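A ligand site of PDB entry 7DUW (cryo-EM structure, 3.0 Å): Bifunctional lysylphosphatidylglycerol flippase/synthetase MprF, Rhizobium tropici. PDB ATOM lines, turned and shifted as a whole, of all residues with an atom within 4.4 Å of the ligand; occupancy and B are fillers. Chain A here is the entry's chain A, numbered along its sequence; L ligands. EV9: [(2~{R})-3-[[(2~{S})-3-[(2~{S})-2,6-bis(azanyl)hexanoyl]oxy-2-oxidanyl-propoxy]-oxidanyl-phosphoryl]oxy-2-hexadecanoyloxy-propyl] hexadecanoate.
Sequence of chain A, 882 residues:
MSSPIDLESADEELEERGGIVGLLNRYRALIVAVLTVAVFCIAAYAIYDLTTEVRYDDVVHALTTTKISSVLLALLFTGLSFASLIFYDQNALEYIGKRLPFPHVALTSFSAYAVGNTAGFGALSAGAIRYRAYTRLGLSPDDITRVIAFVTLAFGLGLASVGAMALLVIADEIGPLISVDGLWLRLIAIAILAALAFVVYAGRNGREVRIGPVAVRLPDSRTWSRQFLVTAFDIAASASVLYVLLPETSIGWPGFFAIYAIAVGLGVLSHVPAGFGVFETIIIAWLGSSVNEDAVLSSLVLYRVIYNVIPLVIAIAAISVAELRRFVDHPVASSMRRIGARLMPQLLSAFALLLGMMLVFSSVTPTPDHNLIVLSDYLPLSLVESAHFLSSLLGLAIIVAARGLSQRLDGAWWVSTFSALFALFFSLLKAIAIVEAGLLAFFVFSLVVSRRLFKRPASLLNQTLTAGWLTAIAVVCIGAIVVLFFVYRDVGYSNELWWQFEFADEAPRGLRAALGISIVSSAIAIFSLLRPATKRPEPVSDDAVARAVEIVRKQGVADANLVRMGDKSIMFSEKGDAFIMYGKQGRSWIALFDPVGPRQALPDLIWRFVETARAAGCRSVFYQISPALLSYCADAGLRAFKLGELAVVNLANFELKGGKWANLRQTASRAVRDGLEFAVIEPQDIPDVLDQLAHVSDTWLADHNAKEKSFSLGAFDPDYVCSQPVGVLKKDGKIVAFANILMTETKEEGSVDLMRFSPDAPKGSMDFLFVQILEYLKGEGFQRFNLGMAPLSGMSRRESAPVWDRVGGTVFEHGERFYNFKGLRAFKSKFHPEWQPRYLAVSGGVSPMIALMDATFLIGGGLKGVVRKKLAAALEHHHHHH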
ATOM      1  N   ILE A  47     -15.699   8.148  11.609  1.00  0.00           N
ATOM      2  CA  ILE A  47     -16.338   6.835  11.631  1.00  0.00           C
ATOM      3  C   ILE A  47     -17.326   6.730  12.774  1.00  0.00           C
ATOM      4  O   ILE A  47     -18.432   6.193  12.621  1.00  0.00           O
ATOM      5  CB  ILE A  47     -15.291   5.698  11.692  1.00  0.00           C
ATOM      6  CG1 ILE A  47     -14.164   5.938  10.712  1.00  0.00           C
ATOM      7  CG2 ILE A  47     -15.947   4.353  11.418  1.00  0.00           C
ATOM      8  CD1 ILE A  47     -13.064   4.910  10.781  1.00  0.00           C
ATOM      9  N   VAL A  60     -21.358  -7.948  13.586  1.00  0.00           N
ATOM     10  CA  VAL A  60     -21.015  -9.366  13.723  1.00  0.00           C
ATOM     11  C   VAL A  60     -21.964 -10.229  12.908  1.00  0.00           C
ATOM     12  O   VAL A  60     -21.559 -11.217  12.281  1.00  0.00           O
ATOM     13  CB  VAL A  60     -20.993  -9.778  15.204  1.00  0.00           C
ATOM     14  CG1 VAL A  60     -20.788 -11.271  15.323  1.00  0.00           C
ATOM     15  CG2 VAL A  60     -19.896  -9.039  15.920  1.00  0.00           C
ATOM     16  N   THR A  64     -20.958 -12.855   9.984  1.00  0.00           N
ATOM     17  CA  THR A  64     -21.292 -14.276   9.960  1.00  0.00           C
ATOM     18  C   THR A  64     -22.065 -14.652   8.712  1.00  0.00           C
ATOM     19  O   THR A  64     -21.951 -15.775   8.227  1.00  0.00           O
ATOM     20  CB  THR A  64     -22.087 -14.658  11.209  1.00  0.00           C
ATOM     21  OG1 THR A  64     -23.309 -13.912  11.246  1.00  0.00           O
ATOM     22  CG2 THR A  64     -21.275 -14.374  12.466  1.00  0.00           C
ATOM     23  N   THR A 118       0.644  -2.821   5.303  1.00  0.00           N
ATOM     24  CA  THR A 118       0.299  -2.978   6.707  1.00  0.00           C
ATOM     25  C   THR A 118       0.940  -1.937   7.604  1.00  0.00           C
ATOM     26  O   THR A 118       0.246  -1.232   8.342  1.00  0.00           O
ATOM     27  CB  THR A 118       0.693  -4.375   7.181  1.00  0.00           C
ATOM     28  OG1 THR A 118      -0.167  -5.354   6.594  1.00  0.00           O
ATOM     29  CG2 THR A 118       0.619  -4.461   8.684  1.00  0.00           C
ATOM     30  N   PRO A 273      -0.552   4.109   9.302  1.00  0.00           N
ATOM     31  CA  PRO A 273      -0.186   2.735   8.899  1.00  0.00           C
ATOM     32  C   PRO A 273      -1.371   2.017   8.264  1.00  0.00           C
ATOM     33  O   PRO A 273      -2.437   1.899   8.863  1.00  0.00           O
ATOM     34  CB  PRO A 273       0.231   2.084  10.225  1.00  0.00           C
ATOM     35  CG  PRO A 273       0.690   3.214  11.061  1.00  0.00           C
ATOM     36  CD  PRO A 273      -0.143   4.405  10.680  1.00  0.00           C
ATOM     37  N   ALA A 274      -1.161   1.566   7.032  1.00  0.00           N
ATOM     38  CA  ALA A 274      -2.160   0.878   6.218  1.00  0.00           C
ATOM     39  C   ALA A 274      -3.360   1.758   5.882  1.00  0.00           C
ATOM     40  O   ALA A 274      -4.375   1.257   5.392  1.00  0.00           O
ATOM     41  CB  ALA A 274      -2.646  -0.414   6.882  1.00  0.00           C
ATOM     42  N   PHE A 276      -5.290   2.871   8.020  1.00  0.00           N
ATOM     43  CA  PHE A 276      -6.298   2.132   8.773  1.00  0.00           C
ATOM     44  C   PHE A 276      -7.475   2.999   9.170  1.00  0.00           C
ATOM     45  O   PHE A 276      -8.608   2.502   9.243  1.00  0.00           O
ATOM     46  CB  PHE A 276      -5.660   1.509  10.026  1.00  0.00           C
ATOM     47  CG  PHE A 276      -6.662   0.978  11.002  1.00  0.00           C
ATOM     48  CD1 PHE A 276      -7.511  -0.045  10.647  1.00  0.00           C
ATOM     49  CD2 PHE A 276      -6.760   1.519  12.264  1.00  0.00           C
ATOM     50  CE1 PHE A 276      -8.433  -0.533  11.536  1.00  0.00           C
ATOM     51  CE2 PHE A 276      -7.678   1.026  13.166  1.00  0.00           C
ATOM     52  CZ  PHE A 276      -8.522   0.007  12.795  1.00  0.00           C
ATOM     53  N   GLU A 280     -11.026   3.490   5.779  1.00  0.00           N
ATOM     54  CA  GLU A 280     -12.342   3.098   6.292  1.00  0.00           C
ATOM     55  C   GLU A 280     -13.242   4.311   6.432  1.00  0.00           C
ATOM     56  O   GLU A 280     -14.448   4.233   6.164  1.00  0.00           O
ATOM     57  CB  GLU A 280     -12.180   2.384   7.627  1.00  0.00           C
ATOM     58  CG  GLU A 280     -11.723   0.934   7.512  1.00  0.00           C
ATOM     59  CD  GLU A 280     -10.231   0.799   7.262  1.00  0.00           C
ATOM     60  OE1 GLU A 280      -9.604   1.756   6.777  1.00  0.00           O
ATOM     61  OE2 GLU A 280      -9.681  -0.277   7.562  1.00  0.00           O
ATOM     62  N   LEU A 297     -19.115  -1.909   7.400  1.00  0.00           N
ATOM     63  CA  LEU A 297     -18.110  -2.139   8.433  1.00  0.00           C
ATOM     64  C   LEU A 297     -17.655  -3.588   8.437  1.00  0.00           C
ATOM     65  O   LEU A 297     -16.456  -3.860   8.604  1.00  0.00           O
ATOM     66  CB  LEU A 297     -18.657  -1.740   9.806  1.00  0.00           C
ATOM     67  CG  LEU A 297     -18.473  -0.270  10.192  1.00  0.00           C
ATOM     68  CD1 LEU A 297     -19.258   0.028  11.444  1.00  0.00           C
ATOM     69  CD2 LEU A 297     -17.001   0.048  10.381  1.00  0.00           C
ATOM     70  N   LEU A 300     -15.402  -4.030   5.506  1.00  0.00           N
ATOM     71  CA  LEU A 300     -14.108  -3.416   5.763  1.00  0.00           C
ATOM     72  C   LEU A 300     -13.265  -4.262   6.699  1.00  0.00           C
ATOM     73  O   LEU A 300     -12.056  -4.412   6.491  1.00  0.00           O
ATOM     74  CB  LEU A 300     -14.296  -2.017   6.348  1.00  0.00           C
ATOM     75  CG  LEU A 300     -14.651  -0.933   5.333  1.00  0.00           C
ATOM     76  CD1 LEU A 300     -15.013   0.349   6.054  1.00  0.00           C
ATOM     77  CD2 LEU A 300     -13.493  -0.708   4.385  1.00  0.00           C
ATOM     78  N   VAL A 301     -13.869  -4.830   7.735  1.00  0.00           N
ATOM     79  CA  VAL A 301     -13.139  -5.704   8.656  1.00  0.00           C
ATOM     80  C   VAL A 301     -12.593  -6.910   7.898  1.00  0.00           C
ATOM     81  O   VAL A 301     -11.424  -7.279   8.030  1.00  0.00           O
ATOM     82  CB  VAL A 301     -14.028  -6.135   9.822  1.00  0.00           C
ATOM     83  CG1 VAL A 301     -13.415  -7.311  10.552  1.00  0.00           C
ATOM     84  CG2 VAL A 301     -14.259  -4.977  10.772  1.00  0.00           C
ATOM     85  N   ARG A 304      -9.788  -5.859   5.499  1.00  0.00           N
ATOM     86  CA  ARG A 304      -8.545  -5.686   6.238  1.00  0.00           C
ATOM     87  C   ARG A 304      -7.925  -7.036   6.556  1.00  0.00           C
ATOM     88  O   ARG A 304      -6.764  -7.283   6.226  1.00  0.00           O
ATOM     89  CB  ARG A 304      -8.788  -4.883   7.515  1.00  0.00           C
ATOM     90  CG  ARG A 304      -8.936  -3.404   7.286  1.00  0.00           C
ATOM     91  CD  ARG A 304      -7.687  -2.829   6.658  1.00  0.00           C
ATOM     92  NE  ARG A 304      -7.766  -1.390   6.518  1.00  0.00           N
ATOM     93  CZ  ARG A 304      -6.872  -0.656   5.869  1.00  0.00           C
ATOM     94  NH1 ARG A 304      -5.828  -1.241   5.295  1.00  0.00           N
ATOM     95  NH2 ARG A 304      -7.016   0.659   5.782  1.00  0.00           N
ATOM     96  N   VAL A 305      -8.717  -7.940   7.136  1.00  0.00           N
ATOM     97  CA  VAL A 305      -8.215  -9.269   7.475  1.00  0.00           C
ATOM     98  C   VAL A 305      -7.582  -9.910   6.254  1.00  0.00           C
ATOM     99  O   VAL A 305      -6.372 -10.162   6.229  1.00  0.00           O
ATOM    100  CB  VAL A 305      -9.349 -10.143   8.037  1.00  0.00           C
ATOM    101  CG1 VAL A 305      -8.934 -11.603   8.050  1.00  0.00           C
ATOM    102  CG2 VAL A 305      -9.702  -9.690   9.440  1.00  0.00           C
ATOM    103  N   ASN A 308      -4.677  -7.720   4.218  1.00  0.00           N
ATOM    104  CA  ASN A 308      -3.490  -7.345   4.968  1.00  0.00           C
ATOM    105  C   ASN A 308      -2.874  -8.504   5.735  1.00  0.00           C
ATOM    106  O   ASN A 308      -1.666  -8.725   5.635  1.00  0.00           O
ATOM    107  CB  ASN A 308      -3.815  -6.203   5.925  1.00  0.00           C
ATOM    108  CG  ASN A 308      -4.161  -4.920   5.208  1.00  0.00           C
ATOM    109  OD1 ASN A 308      -4.768  -4.016   5.788  1.00  0.00           O
ATOM    110  ND2 ASN A 308      -3.784  -4.835   3.947  1.00  0.00           N
ATOM    111  N   VAL A 309      -3.666  -9.240   6.501  1.00  0.00           N
ATOM    112  CA  VAL A 309      -3.114 -10.340   7.285  1.00  0.00           C
ATOM    113  C   VAL A 309      -2.740 -11.517   6.387  1.00  0.00           C
ATOM    114  O   VAL A 309      -1.658 -12.090   6.526  1.00  0.00           O
ATOM    115  CB  VAL A 309      -4.112 -10.750   8.374  1.00  0.00           C
ATOM    116  CG1 VAL A 309      -3.616 -11.977   9.114  1.00  0.00           C
ATOM    117  CG2 VAL A 309      -4.338  -9.606   9.341  1.00  0.00           C
ATOM    118  N   LEU A 353       2.974  -6.549  14.947  1.00  0.00           N
ATOM    119  CA  LEU A 353       2.181  -5.330  15.057  1.00  0.00           C
ATOM    120  C   LEU A 353       0.700  -5.635  14.806  1.00  0.00           C
ATOM    121  O   LEU A 353      -0.170  -5.245  15.593  1.00  0.00           O
ATOM    122  CB  LEU A 353       2.695  -4.271  14.087  1.00  0.00           C
ATOM    123  CG  LEU A 353       1.879  -2.981  14.050  1.00  0.00           C
ATOM    124  CD1 LEU A 353       2.031  -2.233  15.350  1.00  0.00           C
ATOM    125  CD2 LEU A 353       2.312  -2.124  12.882  1.00  0.00           C
ATOM    126  N   LEU A 354       0.411  -6.358  13.721  1.00  0.00           N
ATOM    127  CA  LEU A 354      -0.982  -6.737  13.463  1.00  0.00           C
ATOM    128  C   LEU A 354      -1.534  -7.613  14.567  1.00  0.00           C
ATOM    129  O   LEU A 354      -2.713  -7.495  14.933  1.00  0.00           O
ATOM    130  CB  LEU A 354      -1.113  -7.446  12.123  1.00  0.00           C
ATOM    131  CG  LEU A 354      -1.047  -6.595  10.870  1.00  0.00           C
ATOM    132  CD1 LEU A 354      -1.236  -7.456   9.642  1.00  0.00           C
ATOM    133  CD2 LEU A 354      -2.090  -5.503  10.925  1.00  0.00           C
ATOM    134  N   MET A 357      -2.310  -5.615  17.620  1.00  0.00           N
ATOM    135  CA  MET A 357      -3.514  -4.851  17.299  1.00  0.00           C
ATOM    136  C   MET A 357      -4.758  -5.717  17.436  1.00  0.00           C
ATOM    137  O   MET A 357      -5.775  -5.290  17.998  1.00  0.00           O
ATOM    138  CB  MET A 357      -3.394  -4.292  15.891  1.00  0.00           C
ATOM    139  CG  MET A 357      -4.542  -3.420  15.458  1.00  0.00           C
ATOM    140  SD  MET A 357      -4.239  -2.746  13.816  1.00  0.00           S
ATOM    141  CE  MET A 357      -5.759  -1.878  13.536  1.00  0.00           C
ATOM    142  N   MET A 358      -4.694  -6.949  16.918  1.00  0.00           N
ATOM    143  CA  MET A 358      -5.793  -7.888  17.062  1.00  0.00           C
ATOM    144  C   MET A 358      -6.096  -8.160  18.522  1.00  0.00           C
ATOM    145  O   MET A 358      -7.265  -8.213  18.925  1.00  0.00           O
ATOM    146  CB  MET A 358      -5.460  -9.199  16.355  1.00  0.00           C
ATOM    147  CG  MET A 358      -6.582 -10.213  16.416  1.00  0.00           C
ATOM    148  SD  MET A 358      -6.205 -11.753  15.573  1.00  0.00           S
ATOM    149  CE  MET A 358      -5.005 -12.448  16.689  1.00  0.00           C
ATOM    150  N   PHE A 361      -7.815  -5.094  20.101  1.00  0.00           N
ATOM    151  CA  PHE A 361      -9.184  -4.947  19.612  1.00  0.00           C
ATOM    152  C   PHE A 361     -10.087  -6.030  20.184  1.00  0.00           C
ATOM    153  O   PHE A 361     -11.213  -5.745  20.611  1.00  0.00           O
ATOM    154  CB  PHE A 361      -9.210  -4.979  18.088  1.00  0.00           C
ATOM    155  CG  PHE A 361      -8.952  -3.634  17.458  1.00  0.00           C
ATOM    156  CD1 PHE A 361      -7.964  -2.800  17.953  1.00  0.00           C
ATOM    157  CD2 PHE A 361      -9.696  -3.218  16.374  1.00  0.00           C
ATOM    158  CE1 PHE A 361      -7.731  -1.570  17.367  1.00  0.00           C
ATOM    159  CE2 PHE A 361      -9.464  -1.988  15.788  1.00  0.00           C
ATOM    160  CZ  PHE A 361      -8.475  -1.162  16.287  1.00  0.00           C
ATOM    161  N   SER A 362      -9.607  -7.275  20.216  1.00  0.00           N
ATOM    162  CA  SER A 362     -10.399  -8.366  20.774  1.00  0.00           C
ATOM    163  C   SER A 362     -10.649  -8.176  22.261  1.00  0.00           C
ATOM    164  O   SER A 362     -11.702  -8.568  22.770  1.00  0.00           O
ATOM    165  CB  SER A 362      -9.691  -9.701  20.530  1.00  0.00           C
ATOM    166  OG  SER A 362      -9.812 -10.102  19.183  1.00  0.00           O
ATOM    167  N   THR A 365     -13.477  -5.534  22.044  1.00  0.00           N
ATOM    168  CA  THR A 365     -14.733  -6.076  21.535  1.00  0.00           C
ATOM    169  C   THR A 365     -15.238  -7.217  22.425  1.00  0.00           C
ATOM    170  O   THR A 365     -14.437  -7.964  22.994  1.00  0.00           O
ATOM    171  CB  THR A 365     -14.584  -6.573  20.100  1.00  0.00           C
ATOM    172  OG1 THR A 365     -13.736  -7.714  20.073  1.00  0.00           O
ATOM    173  CG2 THR A 365     -14.019  -5.481  19.212  1.00  0.00           C
ATOM    174  N   PRO A 368     -18.833 -13.440  22.463  1.00  0.00           N
ATOM    175  CA  PRO A 368     -20.208 -13.944  22.381  1.00  0.00           C
ATOM    176  C   PRO A 368     -20.642 -14.589  23.689  1.00  0.00           C
ATOM    177  O   PRO A 368     -19.850 -15.182  24.420  1.00  0.00           O
ATOM    178  CB  PRO A 368     -20.135 -14.971  21.246  1.00  0.00           C
ATOM    179  CG  PRO A 368     -19.034 -14.486  20.387  1.00  0.00           C
ATOM    180  CD  PRO A 368     -18.023 -13.856  21.309  1.00  0.00           C
ATOM    181  N   ALA A 433     -11.961 -18.019  20.946  1.00  0.00           N
ATOM    182  CA  ALA A 433     -10.940 -17.354  20.155  1.00  0.00           C
ATOM    183  C   ALA A 433     -10.183 -18.333  19.250  1.00  0.00           C
ATOM    184  O   ALA A 433      -8.967 -18.491  19.351  1.00  0.00           O
ATOM    185  CB  ALA A 433      -9.978 -16.581  21.058  1.00  0.00           C
ATOM    186  N   ILE A 434     -10.927 -18.996  18.375  1.00  0.00           N
ATOM    187  CA  ILE A 434     -10.324 -20.018  17.526  1.00  0.00           C
ATOM    188  C   ILE A 434      -9.351 -19.395  16.537  1.00  0.00           C
ATOM    189  O   ILE A 434      -8.195 -19.828  16.423  1.00  0.00           O
ATOM    190  CB  ILE A 434     -11.416 -20.834  16.811  1.00  0.00           C
ATOM    191  CG1 ILE A 434     -12.168 -21.696  17.817  1.00  0.00           C
ATOM    192  CG2 ILE A 434     -10.801 -21.697  15.711  1.00  0.00           C
ATOM    193  CD1 ILE A 434     -11.276 -22.632  18.603  1.00  0.00           C
ATOM    194  N   VAL A 435      -9.785 -18.370  15.807  1.00  0.00           N
ATOM    195  CA  VAL A 435      -8.901 -17.736  14.834  1.00  0.00           C
ATOM    196  C   VAL A 435      -7.811 -16.943  15.548  1.00  0.00           C
ATOM    197  O   VAL A 435      -6.659 -16.894  15.094  1.00  0.00           O
ATOM    198  CB  VAL A 435      -9.703 -16.862  13.856  1.00  0.00           C
ATOM    199  CG1 VAL A 435     -10.520 -15.812  14.594  1.00  0.00           C
ATOM    200  CG2 VAL A 435      -8.790 -16.212  12.841  1.00  0.00           C
ATOM    201  N   GLU A 436      -8.149 -16.300  16.671  1.00  0.00           N
ATOM    202  CA  GLU A 436      -7.154 -15.598  17.468  1.00  0.00           C
ATOM    203  C   GLU A 436      -6.065 -16.560  17.933  1.00  0.00           C
ATOM    204  O   GLU A 436      -4.865 -16.278  17.792  1.00  0.00           O
ATOM    205  CB  GLU A 436      -7.827 -14.941  18.660  1.00  0.00           C
ATOM    206  CG  GLU A 436      -7.216 -13.640  19.128  1.00  0.00           C
ATOM    207  CD  GLU A 436      -7.964 -13.044  20.297  1.00  0.00           C
ATOM    208  OE1 GLU A 436      -7.388 -12.965  21.402  1.00  0.00           O
ATOM    209  OE2 GLU A 436      -9.141 -12.689  20.115  1.00  0.00           O
ATOM    210  N   LEU A 439      -3.893 -17.723  14.951  1.00  0.00           N
ATOM    211  CA  LEU A 439      -2.925 -16.719  14.526  1.00  0.00           C
ATOM    212  C   LEU A 439      -1.777 -16.604  15.531  1.00  0.00           C
ATOM    213  O   LEU A 439      -0.613 -16.515  15.135  1.00  0.00           O
ATOM    214  CB  LEU A 439      -3.614 -15.362  14.349  1.00  0.00           C
ATOM    215  CG  LEU A 439      -4.268 -15.151  12.981  1.00  0.00           C
ATOM    216  CD1 LEU A 439      -4.699 -13.705  12.828  1.00  0.00           C
ATOM    217  CD2 LEU A 439      -3.315 -15.546  11.870  1.00  0.00           C
ATOM    218  N   VAL A 475      -2.119   5.024  17.086  1.00  0.00           N
ATOM    219  CA  VAL A 475      -3.205   4.628  16.202  1.00  0.00           C
ATOM    220  C   VAL A 475      -3.935   3.415  16.751  1.00  0.00           C
ATOM    221  O   VAL A 475      -5.174   3.392  16.811  1.00  0.00           O
ATOM    222  CB  VAL A 475      -2.676   4.369  14.777  1.00  0.00           C
ATOM    223  CG1 VAL A 475      -3.701   3.602  13.965  1.00  0.00           C
ATOM    224  CG2 VAL A 475      -2.344   5.672  14.093  1.00  0.00           C
ATOM    225  N   VAL A 476      -3.191   2.407  17.204  1.00  0.00           N
ATOM    226  CA  VAL A 476      -3.824   1.219  17.787  1.00  0.00           C
ATOM    227  C   VAL A 476      -4.644   1.600  19.010  1.00  0.00           C
ATOM    228  O   VAL A 476      -5.779   1.144  19.192  1.00  0.00           O
ATOM    229  CB  VAL A 476      -2.776   0.156  18.118  1.00  0.00           C
ATOM    230  CG1 VAL A 476      -3.408  -0.991  18.881  1.00  0.00           C
ATOM    231  CG2 VAL A 476      -2.131  -0.366  16.843  1.00  0.00           C
ATOM    232  N   GLY A 479      -7.734   3.718  18.094  1.00  0.00           N
ATOM    233  CA  GLY A 479      -8.688   2.830  17.460  1.00  0.00           C
ATOM    234  C   GLY A 479      -9.390   1.937  18.462  1.00  0.00           C
ATOM    235  O   GLY A 479     -10.595   1.703  18.356  1.00  0.00           O
ATOM    236  N   VAL A 483     -13.322   1.984  19.180  1.00  0.00           N
ATOM    237  CA  VAL A 483     -14.081   0.746  19.079  1.00  0.00           C
ATOM    238  C   VAL A 483     -14.832   0.486  20.367  1.00  0.00           C
ATOM    239  O   VAL A 483     -15.963  -0.030  20.354  1.00  0.00           O
ATOM    240  CB  VAL A 483     -13.151  -0.422  18.703  1.00  0.00           C
ATOM    241  CG1 VAL A 483     -13.822  -1.762  18.952  1.00  0.00           C
ATOM    242  CG2 VAL A 483     -12.731  -0.314  17.249  1.00  0.00           C
HETATM  243  C10 EV9 L   1     -10.883  -3.380  10.496  1.00  0.00           C
HETATM  244  C13 EV9 L   1     -10.073  -5.378  13.608  1.00  0.00           C
HETATM  245  C15 EV9 L   1      -9.872  -7.579  14.849  1.00  0.00           C
HETATM  246  C20 EV9 L   1     -11.556 -11.434  15.212  1.00  0.00           C
HETATM  247  C21 EV9 L   1     -12.039 -12.776  15.771  1.00  0.00           C
HETATM  248  C28 EV9 L   1     -14.413 -16.345  16.694  1.00  0.00           C
HETATM  249  C03 EV9 L   1     -11.592   2.493  14.477  1.00  0.00           C
HETATM  250  C04 EV9 L   1     -11.942   1.261  13.640  1.00  0.00           C
HETATM  251  C05 EV9 L   1     -12.339   1.632  12.213  1.00  0.00           C
HETATM  252  C06 EV9 L   1     -11.928   0.555  11.215  1.00  0.00           C
HETATM  253  C07 EV9 L   1     -13.123  -0.260  10.728  1.00  0.00           C
HETATM  254  C08 EV9 L   1     -12.793  -1.737  10.650  1.00  0.00           C
HETATM  255  C09 EV9 L   1     -11.400  -2.001  10.102  1.00  0.00           C
HETATM  256  C11 EV9 L   1     -10.943  -3.606  12.007  1.00  0.00           C
HETATM  257  C12 EV9 L   1     -10.912  -5.090  12.364  1.00  0.00           C
HETATM  258  C14 EV9 L   1     -10.761  -6.366  14.548  1.00  0.00           C
HETATM  259  C16 EV9 L   1     -10.350  -8.352  16.085  1.00  0.00           C
HETATM  260  C19 EV9 L   1     -11.371 -10.461  16.373  1.00  0.00           C
HETATM  261  C27 EV9 L   1     -14.203 -15.596  18.008  1.00  0.00           C
HETATM  262  C29 EV9 L   1     -15.258 -17.592  16.937  1.00  0.00           C
HETATM  263  C31 EV9 L   1     -16.921 -18.221  15.393  1.00  0.00           C
HETATM  264  C33 EV9 L   1     -18.393 -18.415  15.047  1.00  0.00           C
HETATM  265  C34 EV9 L   1     -19.246 -17.920  16.211  1.00  0.00           C
HETATM  266  C35 EV9 L   1     -20.108 -16.718  15.834  1.00  0.00           C
HETATM  267  C36 EV9 L   1     -20.576 -15.940  17.078  1.00  0.00           C
HETATM  268  C37 EV9 L   1     -21.577 -14.832  16.717  1.00  0.00           C
HETATM  269  C42 EV9 L   1     -10.507 -11.551  13.130  1.00  0.00           C
HETATM  270  C44 EV9 L   1      -9.492 -12.249  12.210  1.00  0.00           C
HETATM  271  C45 EV9 L   1      -8.034 -12.057  12.670  1.00  0.00           C
HETATM  272  C46 EV9 L   1      -7.401 -10.807  12.078  1.00  0.00           C
HETATM  273  C47 EV9 L   1      -7.446  -9.626  13.041  1.00  0.00           C
HETATM  274  C48 EV9 L   1      -6.330  -8.608  12.803  1.00  0.00           C
HETATM  275  C49 EV9 L   1      -6.894  -7.263  12.371  1.00  0.00           C
HETATM  276  C50 EV9 L   1      -5.806  -6.271  11.991  1.00  0.00           C
HETATM  277  C51 EV9 L   1      -6.032  -5.660  10.615  1.00  0.00           C
HETATM  278  C52 EV9 L   1      -5.916  -4.153  10.629  1.00  0.00           C
HETATM  279  C53 EV9 L   1      -4.944  -3.643   9.568  1.00  0.00           C
HETATM  280  C54 EV9 L   1      -4.564  -2.188   9.818  1.00  0.00           C
HETATM  281  C55 EV9 L   1      -3.106  -2.038  10.192  1.00  0.00           C
HETATM  282  C56 EV9 L   1      -2.849  -0.790  11.032  1.00  0.00           C
HETATM  283  C57 EV9 L   1      -1.637  -0.949  11.940  1.00  0.00           C
HETATM  284  C58 EV9 L   1      -1.501   0.218  12.913  1.00  0.00           C
HETATM  285  N38 EV9 L   1     -21.854 -14.005  17.889  1.00  0.00           N
HETATM  286  N39 EV9 L   1     -18.650 -19.820  14.808  1.00  0.00           N
HETATM  287  O17 EV9 L   1     -10.875  -7.779  16.981  1.00  0.00           O
HETATM  288  O18 EV9 L   1     -10.166  -9.750  16.152  1.00  0.00           O
HETATM  289  O22 EV9 L   1     -11.412 -12.968  17.021  1.00  0.00           O
HETATM  290  O24 EV9 L   1     -11.287 -15.465  17.660  1.00  0.00           O
HETATM  291  O25 EV9 L   1     -11.766 -13.821  19.436  1.00  0.00           O
HETATM  292  O26 EV9 L   1     -13.610 -14.354  17.708  1.00  0.00           O
HETATM  293  O30 EV9 L   1     -16.551 -17.356  16.434  1.00  0.00           O
HETATM  294  O32 EV9 L   1     -16.088 -18.796  14.786  1.00  0.00           O
HETATM  295  O40 EV9 L   1     -13.166 -16.728  16.178  1.00  0.00           O
HETATM  296  O41 EV9 L   1     -10.361 -11.614  14.528  1.00  0.00           O
HETATM  297  O43 EV9 L   1     -11.414 -10.966  12.659  1.00  0.00           O
HETATM  298  P23 EV9 L   1     -11.992 -14.179  17.987  1.00  0.00           P
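O of Met 358 sits at hydrogen-bond distance from OG of Ser 362, at 3.2 Å.
O of Ser 362 lies close to OG1 of Thr 365 (3.5 Å).
The backbone NH (N) of Ala 274 lies close to the backbone carbonyl oxygen (O) of Thr 118 (3.4 Å).
O of Ala 274 sits at hydrogen-bond distance from NH2 of Arg 304.
The side-chain carboxylate of Glu 436 lies within hydrogen-bond range of the side-chain hydroxyl of Ser 362 (2.8 Å).
The backbone carbonyl oxygen (O) of Phe 361 lies close to the side-chain hydroxyl (OG1) of Thr 365 (3.2 Å).
O of Val 60 lies close to OG1 of Thr 64 (3.4 Å).
The side-chain amide oxygen (OD1) of Asn 308 sits at hydrogen-bond distance from the guanidinium group (NH1) of Arg 304, at 3.0 Å.
Ile 47 touches the ligand.
CG1 of Val 60 touches N38 of the ligand, 3.9 Å away.
Thr 118 touches the ligand.
O of Pro 273 touches C56 of the ligand, 3.5 Å away.
CB of Ala 274 touches C55 of the ligand, at 3.7 Å.
CE1 of Phe 276 touches C09 of the ligand, at 3.6 Å.
Glu 280 touches the ligand.
Leu 297 touches the ligand.
CG2 of Val 301 touches C08 of the ligand (3.6 Å).
Arg 304 touches the ligand (CG to C10, 3.8 Å).
CG2 of Val 305 touches C46 of the ligand, 3.7 Å away.
OD1 of Asn 308 touches C53 of the ligand, at 3.8 Å.
CD2 of Leu 354 touches C53 of the ligand (3.7 Å).
Met 357 touches the ligand.
Met 358 touches the ligand.
Phe 361 touches the ligand.
Pro 368 touches the ligand.
CA of Ala 433 touches O24 of the ligand (3.1 Å).
Ile 434 touches the ligand.
CG1 of Val 435 touches O24 of the ligand, at 3.2 Å.
Leu 439 touches the ligand (CD1 to C45, 3.7 Å).
Hydrophobic or aromatic side chains within 4 Å of the ligand: Ile 47, Val 60, Pro 273, Ala 274, Phe 276, Leu 297, Val 301, Val 305, Leu 354, Met 357, Met 358, Phe 361, Pro 368, Ala 433, Val 435 and Leu 439.
Within 4 Å of the ligand: Ile 47, Val 60, Thr 118, Pro 273, Ala 274, Phe 276, Glu 280, Leu 297, Val 301, Arg 304, Val 305, Asn 308, Leu 354, Met 357, Met 358, Phe 361, Ser 362, Pro 368, Ala 433, Ile 434, Val 435, Glu 436 and Leu 439.
Along chain A the residues within 4 Å of the ligand span positions 47 to 439.
The nearest printed residue that does not touch the ligand is Val 483 (4.02 Å).
OE2 of Glu 436 sits close to O25 of the ligand (2.9 Å).
OG of Ser 362 lies within hydrogen-bond range of O18 of the ligand.
An oxygen (O24) of the ligand sits at hydrogen-bond distance from the backbone NH (N) of Glu 436, 3.4 Å away.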
